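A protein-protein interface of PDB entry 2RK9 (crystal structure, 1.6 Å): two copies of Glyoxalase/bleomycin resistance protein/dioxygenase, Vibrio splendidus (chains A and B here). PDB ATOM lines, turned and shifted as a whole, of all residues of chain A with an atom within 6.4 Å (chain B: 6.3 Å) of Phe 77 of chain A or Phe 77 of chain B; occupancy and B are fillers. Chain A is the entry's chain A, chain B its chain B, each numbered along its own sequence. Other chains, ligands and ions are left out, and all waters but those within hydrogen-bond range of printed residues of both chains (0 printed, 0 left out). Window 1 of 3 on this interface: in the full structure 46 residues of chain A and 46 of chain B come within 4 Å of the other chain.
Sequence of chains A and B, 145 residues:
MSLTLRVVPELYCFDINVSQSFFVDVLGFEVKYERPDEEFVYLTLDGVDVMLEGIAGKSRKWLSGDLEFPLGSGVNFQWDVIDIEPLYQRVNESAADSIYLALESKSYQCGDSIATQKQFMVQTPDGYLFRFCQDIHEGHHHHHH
Val 7 of chain B touches its own counterpart, Val 7 of chain A.
Pro 9 of chain A touches Phe 77 of chain B, and with the chains exchanged Phe 77 of chain A touches Pro 9 of chain B.
Leu 11 of chain A touches Phe 77 of chain B, and with the chains exchanged Phe 77 of chain A touches Leu 11 of chain B.
Val 75 of chain A touches Tyr 128 of chain B, and with the chains exchanged Tyr 128 of chain A touches Val 75 of chain B.
Of the 12 pairs that touch across the chains among the printed residues, 10 have their exchanged pair printed and touching as well.
Among the printed residues, 12 pairs touch across the chains.
Among the printed residues, no Asp or Glu carboxylate lies within 4 Å of a Lys or Arg side-chain nitrogen of the other chain.
Phe 77 of chain A touches just these residues of chain B: Pro 9, Leu 11 and Phe 77.
Of the printed residues of chain A, Val 7 of chain B touches Val 7.
Val 8 of chain B touches none of the printed residues of chain A.
Printed residues of chain A within 4 Å of Pro 9 of chain B: Phe 77 (3.6 Å).
Of the printed residues of chain A, Val 75 of chain B touches Gly 72 and Tyr 128.
Phe 77 of chain B touches just these residues of chain A: Pro 9 (3.7 Å), Leu 11 (3.8 Å) and Phe 77 (3.8 Å).
The nearest residue of chain B that does not touch Phe 77 of chain A is Val 75 of chain B (4.1 Å).
N of Phe 77 of chain A is in hydrogen-bond range of O of Leu 129 of chain A (3.1 Å).
The backbone NH (N) of Arg 131 of chain A is in hydrogen-bond range of the backbone carbonyl oxygen (O) of Phe 77 of chain A (2.8 Å).
The backbone carbonyl oxygen (O) of Leu 129 of chain B is in hydrogen-bond range of the backbone NH (N) of Phe 77 of chain B (3.1 Å).
The backbone carbonyl oxygen (O) of Phe 77 of chain B is in hydrogen-bond range of the backbone NH (N) of Arg 131 of chain B (2.8 Å).
Among the printed residues, pairs that only touch across the chains: Val 7 of chain A with Val 7 of chain B (3.7 Å), Pro 9 of chain A with Phe 77 of chain B (3.7 Å), Leu 11 of chain A with Phe 77 of chain B (3.8 Å), Leu 11 of chain A with Tyr 128 of chain B (3.6 Å), Leu 11 of chain A with Phe 130 of chain B (3.95 Å), Gly 72 of chain A with Val 75 of chain B (3.9 Å), Val 75 of chain A with Tyr 128 of chain B (3.4 Å), Phe 77 of chain A with Pro 9 of chain B (3.6 Å), Phe 77 of chain A with Leu 11 of chain B (3.8 Å), Phe 77 of chain A with Phe 77 of chain B (3.8 Å), Tyr 128 of chain A with Leu 11 of chain B (3.5 Å) and Tyr 128 of chain A with Val 75 of chain B (3.5 Å).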
ATOM      1  N   VAL A   7      -4.524  -8.814   1.364  1.00  0.00           N
ATOM      2  CA  VAL A   7      -4.755  -7.815   0.347  1.00  0.00           C
ATOM      3  C   VAL A   7      -5.871  -8.457  -0.460  1.00  0.00           C
ATOM      4  O   VAL A   7      -5.784  -9.622  -0.835  1.00  0.00           O
ATOM      5  CB  VAL A   7      -3.528  -7.550  -0.571  1.00  0.00           C
ATOM      6  CG1 VAL A   7      -3.001  -8.846  -1.152  1.00  0.00           C
ATOM      7  CG2 VAL A   7      -3.941  -6.597  -1.706  1.00  0.00           C
ATOM      8  N   VAL A   8      -6.952  -7.723  -0.670  1.00  0.00           N
ATOM      9  CA  VAL A   8      -8.056  -8.259  -1.443  1.00  0.00           C
ATOM     10  C   VAL A   8      -8.210  -7.393  -2.676  1.00  0.00           C
ATOM     11  O   VAL A   8      -8.600  -6.235  -2.584  1.00  0.00           O
ATOM     12  CB  VAL A   8      -9.387  -8.243  -0.659  1.00  0.00           C
ATOM     13  CG1 VAL A   8     -10.506  -8.766  -1.560  1.00  0.00           C
ATOM     14  CG2 VAL A   8      -9.284  -9.122   0.584  1.00  0.00           C
ATOM     15  N   PRO A   9      -7.890  -7.942  -3.851  1.00  0.00           N
ATOM     16  CA  PRO A   9      -8.023  -7.135  -5.065  1.00  0.00           C
ATOM     17  C   PRO A   9      -9.485  -6.862  -5.384  1.00  0.00           C
ATOM     18  O   PRO A   9     -10.343  -7.718  -5.196  1.00  0.00           O
ATOM     19  CB  PRO A   9      -7.369  -8.008  -6.141  1.00  0.00           C
ATOM     20  CG  PRO A   9      -6.412  -8.881  -5.360  1.00  0.00           C
ATOM     21  CD  PRO A   9      -7.221  -9.223  -4.138  1.00  0.00           C
ATOM     22  N   GLU A  10      -9.760  -5.650  -5.837  1.00  0.00           N
ATOM     23  CA  GLU A  10     -11.103  -5.282  -6.243  1.00  0.00           C
ATOM     24  C   GLU A  10     -10.955  -5.049  -7.735  1.00  0.00           C
ATOM     25  O   GLU A  10     -10.193  -4.186  -8.167  1.00  0.00           O
ATOM     26  CB  GLU A  10     -11.563  -4.010  -5.543  1.00  0.00           C
ATOM     27  CG  GLU A  10     -12.729  -3.354  -6.241  1.00  0.00           C
ATOM     28  CD  GLU A  10     -13.431  -2.340  -5.374  1.00  0.00           C
ATOM     29  OE1 GLU A  10     -12.738  -1.591  -4.652  1.00  0.00           O
ATOM     30  OE2 GLU A  10     -14.680  -2.300  -5.427  1.00  0.00           O
ATOM     31  N   LEU A  11     -11.659  -5.855  -8.520  1.00  0.00           N
ATOM     32  CA  LEU A  11     -11.580  -5.763  -9.972  1.00  0.00           C
ATOM     33  C   LEU A  11     -12.819  -5.173 -10.606  1.00  0.00           C
ATOM     34  O   LEU A  11     -13.941  -5.617 -10.349  1.00  0.00           O
ATOM     35  CB  LEU A  11     -11.341  -7.148 -10.565  1.00  0.00           C
ATOM     36  CG  LEU A  11     -10.193  -7.932  -9.927  1.00  0.00           C
ATOM     37  CD1 LEU A  11     -10.121  -9.313 -10.548  1.00  0.00           C
ATOM     38  CD2 LEU A  11      -8.880  -7.189 -10.112  1.00  0.00           C
ATOM     39  N   GLY A  72      -2.144  -1.383 -14.286  1.00  0.00           N
ATOM     40  CA  GLY A  72      -3.138  -1.853 -13.335  1.00  0.00           C
ATOM     41  C   GLY A  72      -4.550  -1.297 -13.460  1.00  0.00           C
ATOM     42  O   GLY A  72      -5.322  -1.366 -12.511  1.00  0.00           O
ATOM     43  N   VAL A  75      -7.946  -2.220 -11.382  1.00  0.00           N
ATOM     44  CA  VAL A  75      -7.617  -2.898 -10.131  1.00  0.00           C
ATOM     45  C   VAL A  75      -7.394  -1.924  -8.996  1.00  0.00           C
ATOM     46  O   VAL A  75      -6.744  -0.911  -9.175  1.00  0.00           O
ATOM     47  CB  VAL A  75      -6.331  -3.717 -10.251  1.00  0.00           C
ATOM     48  CG1 VAL A  75      -6.031  -4.397  -8.908  1.00  0.00           C
ATOM     49  CG2 VAL A  75      -6.468  -4.725 -11.365  1.00  0.00           C
ATOM     50  N   ASN A  76      -7.941  -2.247  -7.832  1.00  0.00           N
ATOM     51  CA  ASN A  76      -7.770  -1.434  -6.640  1.00  0.00           C
ATOM     52  C   ASN A  76      -7.401  -2.432  -5.557  1.00  0.00           C
ATOM     53  O   ASN A  76      -8.212  -3.277  -5.193  1.00  0.00           O
ATOM     54  CB  ASN A  76      -9.061  -0.705  -6.255  1.00  0.00           C
ATOM     55  CG  ASN A  76      -8.971  -0.071  -4.890  1.00  0.00           C
ATOM     56  OD1 ASN A  76      -7.952   0.541  -4.543  1.00  0.00           O
ATOM     57  ND2 ASN A  76     -10.038  -0.208  -4.097  1.00  0.00           N
ATOM     58  N   PHE A  77      -6.173  -2.340  -5.056  1.00  0.00           N
ATOM     59  CA  PHE A  77      -5.709  -3.268  -4.035  1.00  0.00           C
ATOM     60  C   PHE A  77      -6.162  -2.886  -2.631  1.00  0.00           C
ATOM     61  O   PHE A  77      -5.582  -1.985  -2.027  1.00  0.00           O
ATOM     62  CB  PHE A  77      -4.179  -3.339  -4.066  1.00  0.00           C
ATOM     63  CG  PHE A  77      -3.621  -3.884  -5.346  1.00  0.00           C
ATOM     64  CD1 PHE A  77      -3.678  -5.245  -5.619  1.00  0.00           C
ATOM     65  CD2 PHE A  77      -3.034  -3.036  -6.279  1.00  0.00           C
ATOM     66  CE1 PHE A  77      -3.158  -5.756  -6.801  1.00  0.00           C
ATOM     67  CE2 PHE A  77      -2.509  -3.541  -7.471  1.00  0.00           C
ATOM     68  CZ  PHE A  77      -2.573  -4.907  -7.727  1.00  0.00           C
ATOM     69  N   GLN A  78      -7.194  -3.549  -2.112  1.00  0.00           N
ATOM     70  CA  GLN A  78      -7.642  -3.260  -0.748  1.00  0.00           C
ATOM     71  C   GLN A  78      -6.622  -3.969   0.145  1.00  0.00           C
ATOM     72  O   GLN A  78      -6.630  -5.191   0.260  1.00  0.00           O
ATOM     73  CB  GLN A  78      -9.047  -3.812  -0.483  1.00  0.00           C
ATOM     74  CG  GLN A  78      -9.476  -3.590   0.964  1.00  0.00           C
ATOM     75  CD  GLN A  78     -10.828  -4.188   1.307  1.00  0.00           C
ATOM     76  OE1 GLN A  78     -11.870  -3.719   0.838  1.00  0.00           O
ATOM     77  NE2 GLN A  78     -10.818  -5.237   2.134  1.00  0.00           N
ATOM     78  N   TRP A  79      -5.764  -3.185   0.790  1.00  0.00           N
ATOM     79  CA  TRP A  79      -4.674  -3.721   1.599  1.00  0.00           C
ATOM     80  C   TRP A  79      -4.773  -3.501   3.117  1.00  0.00           C
ATOM     81  O   TRP A  79      -4.681  -2.368   3.591  1.00  0.00           O
ATOM     82  CB  TRP A  79      -3.378  -3.107   1.058  1.00  0.00           C
ATOM     83  CG  TRP A  79      -2.110  -3.715   1.532  1.00  0.00           C
ATOM     84  CD1 TRP A  79      -1.600  -3.671   2.795  1.00  0.00           C
ATOM     85  CD2 TRP A  79      -1.150  -4.420   0.734  1.00  0.00           C
ATOM     86  NE1 TRP A  79      -0.379  -4.297   2.836  1.00  0.00           N
ATOM     87  CE2 TRP A  79      -0.077  -4.767   1.586  1.00  0.00           C
ATOM     88  CE3 TRP A  79      -1.090  -4.790  -0.617  1.00  0.00           C
ATOM     89  CZ2 TRP A  79       1.042  -5.468   1.132  1.00  0.00           C
ATOM     90  CZ3 TRP A  79       0.024  -5.489  -1.069  1.00  0.00           C
ATOM     91  CH2 TRP A  79       1.078  -5.820  -0.193  1.00  0.00           C
ATOM     92  N   TYR A 128      -0.262   1.989 -10.183  1.00  0.00           N
ATOM     93  CA  TYR A 128      -1.078   1.097  -9.370  1.00  0.00           C
ATOM     94  C   TYR A 128      -1.728   1.832  -8.201  1.00  0.00           C
ATOM     95  O   TYR A 128      -1.097   2.669  -7.552  1.00  0.00           O
ATOM     96  CB  TYR A 128      -0.218  -0.058  -8.844  1.00  0.00           C
ATOM     97  CG  TYR A 128       0.444  -0.869  -9.936  1.00  0.00           C
ATOM     98  CD1 TYR A 128      -0.319  -1.610 -10.834  1.00  0.00           C
ATOM     99  CD2 TYR A 128       1.834  -0.889 -10.074  1.00  0.00           C
ATOM    100  CE1 TYR A 128       0.286  -2.354 -11.846  1.00  0.00           C
ATOM    101  CE2 TYR A 128       2.450  -1.628 -11.087  1.00  0.00           C
ATOM    102  CZ  TYR A 128       1.669  -2.357 -11.966  1.00  0.00           C
ATOM    103  OH  TYR A 128       2.267  -3.088 -12.963  1.00  0.00           O
ATOM    104  N   LEU A 129      -2.992   1.512  -7.934  1.00  0.00           N
ATOM    105  CA  LEU A 129      -3.717   2.157  -6.843  1.00  0.00           C
ATOM    106  C   LEU A 129      -3.914   1.213  -5.666  1.00  0.00           C
ATOM    107  O   LEU A 129      -4.397   0.093  -5.814  1.00  0.00           O
ATOM    108  CB  LEU A 129      -5.078   2.677  -7.330  1.00  0.00           C
ATOM    109  CG  LEU A 129      -5.041   3.702  -8.469  1.00  0.00           C
ATOM    110  CD1 LEU A 129      -6.451   4.014  -8.972  1.00  0.00           C
ATOM    111  CD2 LEU A 129      -4.377   4.970  -7.964  1.00  0.00           C
ATOM    112  N   PHE A 130      -3.514   1.685  -4.493  1.00  0.00           N
ATOM    113  CA  PHE A 130      -3.618   0.923  -3.265  1.00  0.00           C
ATOM    114  C   PHE A 130      -4.561   1.610  -2.297  1.00  0.00           C
ATOM    115  O   PHE A 130      -4.481   2.817  -2.073  1.00  0.00           O
ATOM    116  CB  PHE A 130      -2.238   0.786  -2.612  1.00  0.00           C
ATOM    117  CG  PHE A 130      -1.365  -0.266  -3.241  1.00  0.00           C
ATOM    118  CD1 PHE A 130      -1.130  -1.473  -2.590  1.00  0.00           C
ATOM    119  CD2 PHE A 130      -0.790  -0.059  -4.488  1.00  0.00           C
ATOM    120  CE1 PHE A 130      -0.330  -2.460  -3.173  1.00  0.00           C
ATOM    121  CE2 PHE A 130       0.012  -1.042  -5.079  1.00  0.00           C
ATOM    122  CZ  PHE A 130       0.241  -2.241  -4.422  1.00  0.00           C
ATOM    123  N   ARG A 131      -5.467   0.822  -1.733  1.00  0.00           N
ATOM    124  CA  ARG A 131      -6.404   1.332  -0.757  1.00  0.00           C
ATOM    125  C   ARG A 131      -6.031   0.675   0.576  1.00  0.00           C
ATOM    126  O   ARG A 131      -6.410  -0.467   0.846  1.00  0.00           O
ATOM    127  CB  ARG A 131      -7.838   0.961  -1.148  1.00  0.00           C
ATOM    128  CG  ARG A 131      -8.888   1.476  -0.173  1.00  0.00           C
ATOM    129  CD  ARG A 131     -10.272   0.864  -0.427  1.00  0.00           C
ATOM    130  NE  ARG A 131     -10.779   1.137  -1.758  1.00  0.00           N
ATOM    131  CZ  ARG A 131     -12.062   1.065  -2.108  1.00  0.00           C
ATOM    132  NH1 ARG A 131     -12.989   0.724  -1.216  1.00  0.00           N
ATOM    133  NH2 ARG A 131     -12.427   1.344  -3.362  1.00  0.00           N
ATOM    134  N   PHE A 132      -5.268   1.396   1.393  1.00  0.00           N
ATOM    135  CA  PHE A 132      -4.862   0.879   2.691  1.00  0.00           C
ATOM    136  C   PHE A 132      -6.036   1.004   3.652  1.00  0.00           C
ATOM    137  O   PHE A 132      -6.621   2.079   3.800  1.00  0.00           O
ATOM    138  CB  PHE A 132      -3.622   1.638   3.184  1.00  0.00           C
ATOM    139  CG  PHE A 132      -2.399   1.385   2.338  1.00  0.00           C
ATOM    140  CD1 PHE A 132      -1.824   0.114   2.288  1.00  0.00           C
ATOM    141  CD2 PHE A 132      -1.877   2.389   1.526  1.00  0.00           C
ATOM    142  CE1 PHE A 132      -0.748  -0.156   1.432  1.00  0.00           C
ATOM    143  CE2 PHE A 132      -0.806   2.129   0.672  1.00  0.00           C
ATOM    144  CZ  PHE A 132      -0.241   0.857   0.623  1.00  0.00           C
ATOM    145  N   CYS A 133      -6.388  -0.113   4.287  1.00  0.00           N
ATOM    146  CA  CYS A 133      -7.530  -0.155   5.198  1.00  0.00           C
ATOM    147  C   CYS A 133      -7.218  -0.780   6.538  1.00  0.00           C
ATOM    148  O   CYS A 133      -6.293  -1.577   6.666  1.00  0.00           O
ATOM    149  CB  CYS A 133      -8.667  -0.989   4.602  1.00  0.00           C
ATOM    150  SG  CYS A 133      -9.054  -0.695   2.899  1.00  0.00           S
ATOM    151  N   VAL B   7      -3.132 -14.578  -2.111  1.00  0.00           N
ATOM    152  CA  VAL B   7      -2.972 -14.122  -3.479  1.00  0.00           C
ATOM    153  C   VAL B   7      -1.886 -13.070  -3.347  1.00  0.00           C
ATOM    154  O   VAL B   7      -1.990 -12.173  -2.515  1.00  0.00           O
ATOM    155  CB  VAL B   7      -4.248 -13.471  -4.085  1.00  0.00           C
ATOM    156  CG1 VAL B   7      -4.761 -12.332  -3.207  1.00  0.00           C
ATOM    157  CG2 VAL B   7      -3.915 -12.936  -5.478  1.00  0.00           C
ATOM    158  N   VAL B   8      -0.823 -13.210  -4.130  1.00  0.00           N
ATOM    159  CA  VAL B   8       0.273 -12.258  -4.094  1.00  0.00           C
ATOM    160  C   VAL B   8       0.375 -11.614  -5.466  1.00  0.00           C
ATOM    161  O   VAL B   8       0.704 -12.263  -6.451  1.00  0.00           O
ATOM    162  CB  VAL B   8       1.625 -12.939  -3.747  1.00  0.00           C
ATOM    163  CG1 VAL B   8       2.733 -11.887  -3.666  1.00  0.00           C
ATOM    164  CG2 VAL B   8       1.515 -13.682  -2.416  1.00  0.00           C
ATOM    165  N   PRO B   9       0.052 -10.325  -5.549  1.00  0.00           N
ATOM    166  CA  PRO B   9       0.123  -9.629  -6.832  1.00  0.00           C
ATOM    167  C   PRO B   9       1.564  -9.434  -7.269  1.00  0.00           C
ATOM    168  O   PRO B   9       2.435  -9.154  -6.451  1.00  0.00           O
ATOM    169  CB  PRO B   9      -0.551  -8.290  -6.538  1.00  0.00           C
ATOM    170  CG  PRO B   9      -1.461  -8.596  -5.384  1.00  0.00           C
ATOM    171  CD  PRO B   9      -0.591  -9.479  -4.531  1.00  0.00           C
ATOM    172  N   GLU B  10       1.813  -9.613  -8.558  1.00  0.00           N
ATOM    173  CA  GLU B  10       3.140  -9.375  -9.097  1.00  0.00           C
ATOM    174  C   GLU B  10       2.933  -8.191 -10.025  1.00  0.00           C
ATOM    175  O   GLU B  10       2.099  -8.241 -10.926  1.00  0.00           O
ATOM    176  CB  GLU B  10       3.658 -10.580  -9.873  1.00  0.00           C
ATOM    177  CG  GLU B  10       4.984 -10.305 -10.563  1.00  0.00           C
ATOM    178  CD  GLU B  10       5.646 -11.561 -11.085  1.00  0.00           C
ATOM    179  OE1 GLU B  10       4.933 -12.402 -11.665  1.00  0.00           O
ATOM    180  OE2 GLU B  10       6.881 -11.695 -10.916  1.00  0.00           O
ATOM    181  N   LEU B  11       3.688  -7.125  -9.792  1.00  0.00           N
ATOM    182  CA  LEU B  11       3.546  -5.902 -10.574  1.00  0.00           C
ATOM    183  C   LEU B  11       4.726  -5.582 -11.480  1.00  0.00           C
ATOM    184  O   LEU B  11       5.873  -5.606 -11.044  1.00  0.00           O
ATOM    185  CB  LEU B  11       3.347  -4.722  -9.621  1.00  0.00           C
ATOM    186  CG  LEU B  11       2.369  -4.918  -8.463  1.00  0.00           C
ATOM    187  CD1 LEU B  11       2.397  -3.680  -7.571  1.00  0.00           C
ATOM    188  CD2 LEU B  11       0.969  -5.180  -9.004  1.00  0.00           C
ATOM    189  N   GLY B  72      -6.085  -4.407 -16.176  1.00  0.00           N
ATOM    190  CA  GLY B  72      -5.034  -4.955 -15.332  1.00  0.00           C
ATOM    191  C   GLY B  72      -3.647  -5.114 -15.931  1.00  0.00           C
ATOM    192  O   GLY B  72      -2.842  -5.890 -15.415  1.00  0.00           O
ATOM    193  N   VAL B  75      -0.209  -6.472 -14.266  1.00  0.00           N
ATOM    194  CA  VAL B  75      -0.483  -7.256 -13.063  1.00  0.00           C
ATOM    195  C   VAL B  75      -0.717  -8.743 -13.319  1.00  0.00           C
ATOM    196  O   VAL B  75      -1.424  -9.133 -14.250  1.00  0.00           O
ATOM    197  CB  VAL B  75      -1.712  -6.721 -12.300  1.00  0.00           C
ATOM    198  CG1 VAL B  75      -1.808  -7.385 -10.934  1.00  0.00           C
ATOM    199  CG2 VAL B  75      -1.612  -5.233 -12.144  1.00  0.00           C
ATOM    200  N   ASN B  76      -0.111  -9.557 -12.468  1.00  0.00           N
ATOM    201  CA  ASN B  76      -0.260 -10.998 -12.528  1.00  0.00           C
ATOM    202  C   ASN B  76      -0.565 -11.401 -11.087  1.00  0.00           C
ATOM    203  O   ASN B  76       0.227 -11.132 -10.184  1.00  0.00           O
ATOM    204  CB  ASN B  76       1.029 -11.656 -13.025  1.00  0.00           C
ATOM    205  CG  ASN B  76       1.003 -13.157 -12.886  1.00  0.00           C
ATOM    206  OD1 ASN B  76       0.070 -13.818 -13.339  1.00  0.00           O
ATOM    207  ND2 ASN B  76       2.038 -13.712 -12.256  1.00  0.00           N
ATOM    208  N   PHE B  77      -1.733 -12.000 -10.870  1.00  0.00           N
ATOM    209  CA  PHE B  77      -2.144 -12.419  -9.533  1.00  0.00           C
ATOM    210  C   PHE B  77      -1.673 -13.841  -9.233  1.00  0.00           C
ATOM    211  O   PHE B  77      -2.213 -14.792  -9.786  1.00  0.00           O
ATOM    212  CB  PHE B  77      -3.672 -12.366  -9.415  1.00  0.00           C
ATOM    213  CG  PHE B  77      -4.249 -10.979  -9.539  1.00  0.00           C
ATOM    214  CD1 PHE B  77      -4.150 -10.070  -8.487  1.00  0.00           C
ATOM    215  CD2 PHE B  77      -4.884 -10.578 -10.712  1.00  0.00           C
ATOM    216  CE1 PHE B  77      -4.676  -8.781  -8.600  1.00  0.00           C
ATOM    217  CE2 PHE B  77      -5.413  -9.289 -10.837  1.00  0.00           C
ATOM    218  CZ  PHE B  77      -5.306  -8.389  -9.773  1.00  0.00           C
ATOM    219  N   GLN B  78      -0.660 -13.983  -8.381  1.00  0.00           N
ATOM    220  CA  GLN B  78      -0.175 -15.312  -8.013  1.00  0.00           C
ATOM    221  C   GLN B  78      -1.143 -15.777  -6.938  1.00  0.00           C
ATOM    222  O   GLN B  78      -1.080 -15.334  -5.791  1.00  0.00           O
ATOM    223  CB  GLN B  78       1.246 -15.257  -7.466  1.00  0.00           C
ATOM    224  CG  GLN B  78       1.727 -16.601  -6.932  1.00  0.00           C
ATOM    225  CD  GLN B  78       3.171 -16.563  -6.477  1.00  0.00           C
ATOM    226  OE1 GLN B  78       4.090 -16.554  -7.296  1.00  0.00           O
ATOM    227  NE2 GLN B  78       3.381 -16.529  -5.161  1.00  0.00           N
ATOM    228  N   TRP B  79      -2.018 -16.696  -7.329  1.00  0.00           N
ATOM    229  CA  TRP B  79      -3.088 -17.189  -6.478  1.00  0.00           C
ATOM    230  C   TRP B  79      -2.940 -18.633  -6.012  1.00  0.00           C
ATOM    231  O   TRP B  79      -3.008 -19.558  -6.825  1.00  0.00           O
ATOM    232  CB  TRP B  79      -4.388 -17.020  -7.261  1.00  0.00           C
ATOM    233  CG  TRP B  79      -5.633 -17.227  -6.484  1.00  0.00           C
ATOM    234  CD1 TRP B  79      -6.091 -18.401  -5.972  1.00  0.00           C
ATOM    235  CD2 TRP B  79      -6.605 -16.231  -6.150  1.00  0.00           C
ATOM    236  NE1 TRP B  79      -7.297 -18.202  -5.337  1.00  0.00           N
ATOM    237  CE2 TRP B  79      -7.633 -16.877  -5.431  1.00  0.00           C
ATOM    238  CE3 TRP B  79      -6.706 -14.852  -6.386  1.00  0.00           C
ATOM    239  CZ2 TRP B  79      -8.751 -16.196  -4.945  1.00  0.00           C
ATOM    240  CZ3 TRP B  79      -7.822 -14.174  -5.899  1.00  0.00           C
ATOM    241  CH2 TRP B  79      -8.826 -14.850  -5.186  1.00  0.00           C
ATOM    242  N   TYR B 128      -7.892  -9.627 -16.942  1.00  0.00           N
ATOM    243  CA  TYR B 128      -7.020  -9.898 -15.793  1.00  0.00           C
ATOM    244  C   TYR B 128      -6.317 -11.250 -15.878  1.00  0.00           C
ATOM    245  O   TYR B 128      -6.914 -12.254 -16.260  1.00  0.00           O
ATOM    246  CB  TYR B 128      -7.821  -9.835 -14.492  1.00  0.00           C
ATOM    247  CG  TYR B 128      -8.484  -8.504 -14.261  1.00  0.00           C
ATOM    248  CD1 TYR B 128      -7.727  -7.356 -14.006  1.00  0.00           C
ATOM    249  CD2 TYR B 128      -9.873  -8.382 -14.298  1.00  0.00           C
ATOM    250  CE1 TYR B 128      -8.336  -6.132 -13.798  1.00  0.00           C
ATOM    251  CE2 TYR B 128     -10.488  -7.155 -14.087  1.00  0.00           C
ATOM    252  CZ  TYR B 128      -9.714  -6.040 -13.839  1.00  0.00           C
ATOM    253  OH  TYR B 128     -10.312  -4.825 -13.637  1.00  0.00           O
ATOM    254  N   LEU B 129      -5.040 -11.273 -15.511  1.00  0.00           N
ATOM    255  CA  LEU B 129      -4.278 -12.510 -15.553  1.00  0.00           C
ATOM    256  C   LEU B 129      -4.078 -13.094 -14.164  1.00  0.00           C
ATOM    257  O   LEU B 129      -3.593 -12.412 -13.261  1.00  0.00           O
ATOM    258  CB  LEU B 129      -2.918 -12.272 -16.201  1.00  0.00           C
ATOM    259  CG  LEU B 129      -2.946 -11.951 -17.693  1.00  0.00           C
ATOM    260  CD1 LEU B 129      -1.532 -11.632 -18.152  1.00  0.00           C
ATOM    261  CD2 LEU B 129      -3.508 -13.144 -18.468  1.00  0.00           C
ATOM    262  N   PHE B 130      -4.470 -14.358 -14.011  1.00  0.00           N
ATOM    263  CA  PHE B 130      -4.337 -15.084 -12.754  1.00  0.00           C
ATOM    264  C   PHE B 130      -3.380 -16.250 -12.952  1.00  0.00           C
ATOM    265  O   PHE B 130      -3.516 -17.021 -13.905  1.00  0.00           O
ATOM    266  CB  PHE B 130      -5.693 -15.645 -12.307  1.00  0.00           C
ATOM    267  CG  PHE B 130      -6.588 -14.640 -11.629  1.00  0.00           C
ATOM    268  CD1 PHE B 130      -6.864 -14.749 -10.270  1.00  0.00           C
ATOM    269  CD2 PHE B 130      -7.173 -13.607 -12.348  1.00  0.00           C
ATOM    270  CE1 PHE B 130      -7.711 -13.839  -9.635  1.00  0.00           C
ATOM    271  CE2 PHE B 130      -8.014 -12.697 -11.729  1.00  0.00           C
ATOM    272  CZ  PHE B 130      -8.289 -12.811 -10.368  1.00  0.00           C
ATOM    273  N   ARG B 131      -2.409 -16.375 -12.058  1.00  0.00           N
ATOM    274  CA  ARG B 131      -1.471 -17.486 -12.121  1.00  0.00           C
ATOM    275  C   ARG B 131      -1.789 -18.342 -10.904  1.00  0.00           C
ATOM    276  O   ARG B 131      -1.370 -18.029  -9.790  1.00  0.00           O
ATOM    277  CB  ARG B 131      -0.024 -16.997 -12.038  1.00  0.00           C
ATOM    278  CG  ARG B 131       1.000 -18.114 -12.173  1.00  0.00           C
ATOM    279  CD  ARG B 131       2.260 -17.803 -11.389  1.00  0.00           C
ATOM    280  NE  ARG B 131       2.883 -16.529 -11.758  1.00  0.00           N
ATOM    281  CZ  ARG B 131       3.766 -16.383 -12.741  1.00  0.00           C
ATOM    282  NH1 ARG B 131       4.133 -17.431 -13.466  1.00  0.00           N
ATOM    283  NH2 ARG B 131       4.305 -15.193 -12.984  1.00  0.00           N
ATOM    284  N   PHE B 132      -2.559 -19.404 -11.113  1.00  0.00           N
ATOM    285  CA  PHE B 132      -2.926 -20.291 -10.015  1.00  0.00           C
ATOM    286  C   PHE B 132      -1.748 -21.200  -9.706  1.00  0.00           C
ATOM    287  O   PHE B 132      -1.124 -21.748 -10.616  1.00  0.00           O
ATOM    288  CB  PHE B 132      -4.173 -21.094 -10.395  1.00  0.00           C
ATOM    289  CG  PHE B 132      -5.418 -20.258 -10.468  1.00  0.00           C
ATOM    290  CD1 PHE B 132      -5.966 -19.713  -9.313  1.00  0.00           C
ATOM    291  CD2 PHE B 132      -6.013 -19.968 -11.695  1.00  0.00           C
ATOM    292  CE1 PHE B 132      -7.086 -18.892  -9.374  1.00  0.00           C
ATOM    293  CE2 PHE B 132      -7.135 -19.146 -11.763  1.00  0.00           C
ATOM    294  CZ  PHE B 132      -7.669 -18.606 -10.601  1.00  0.00           C
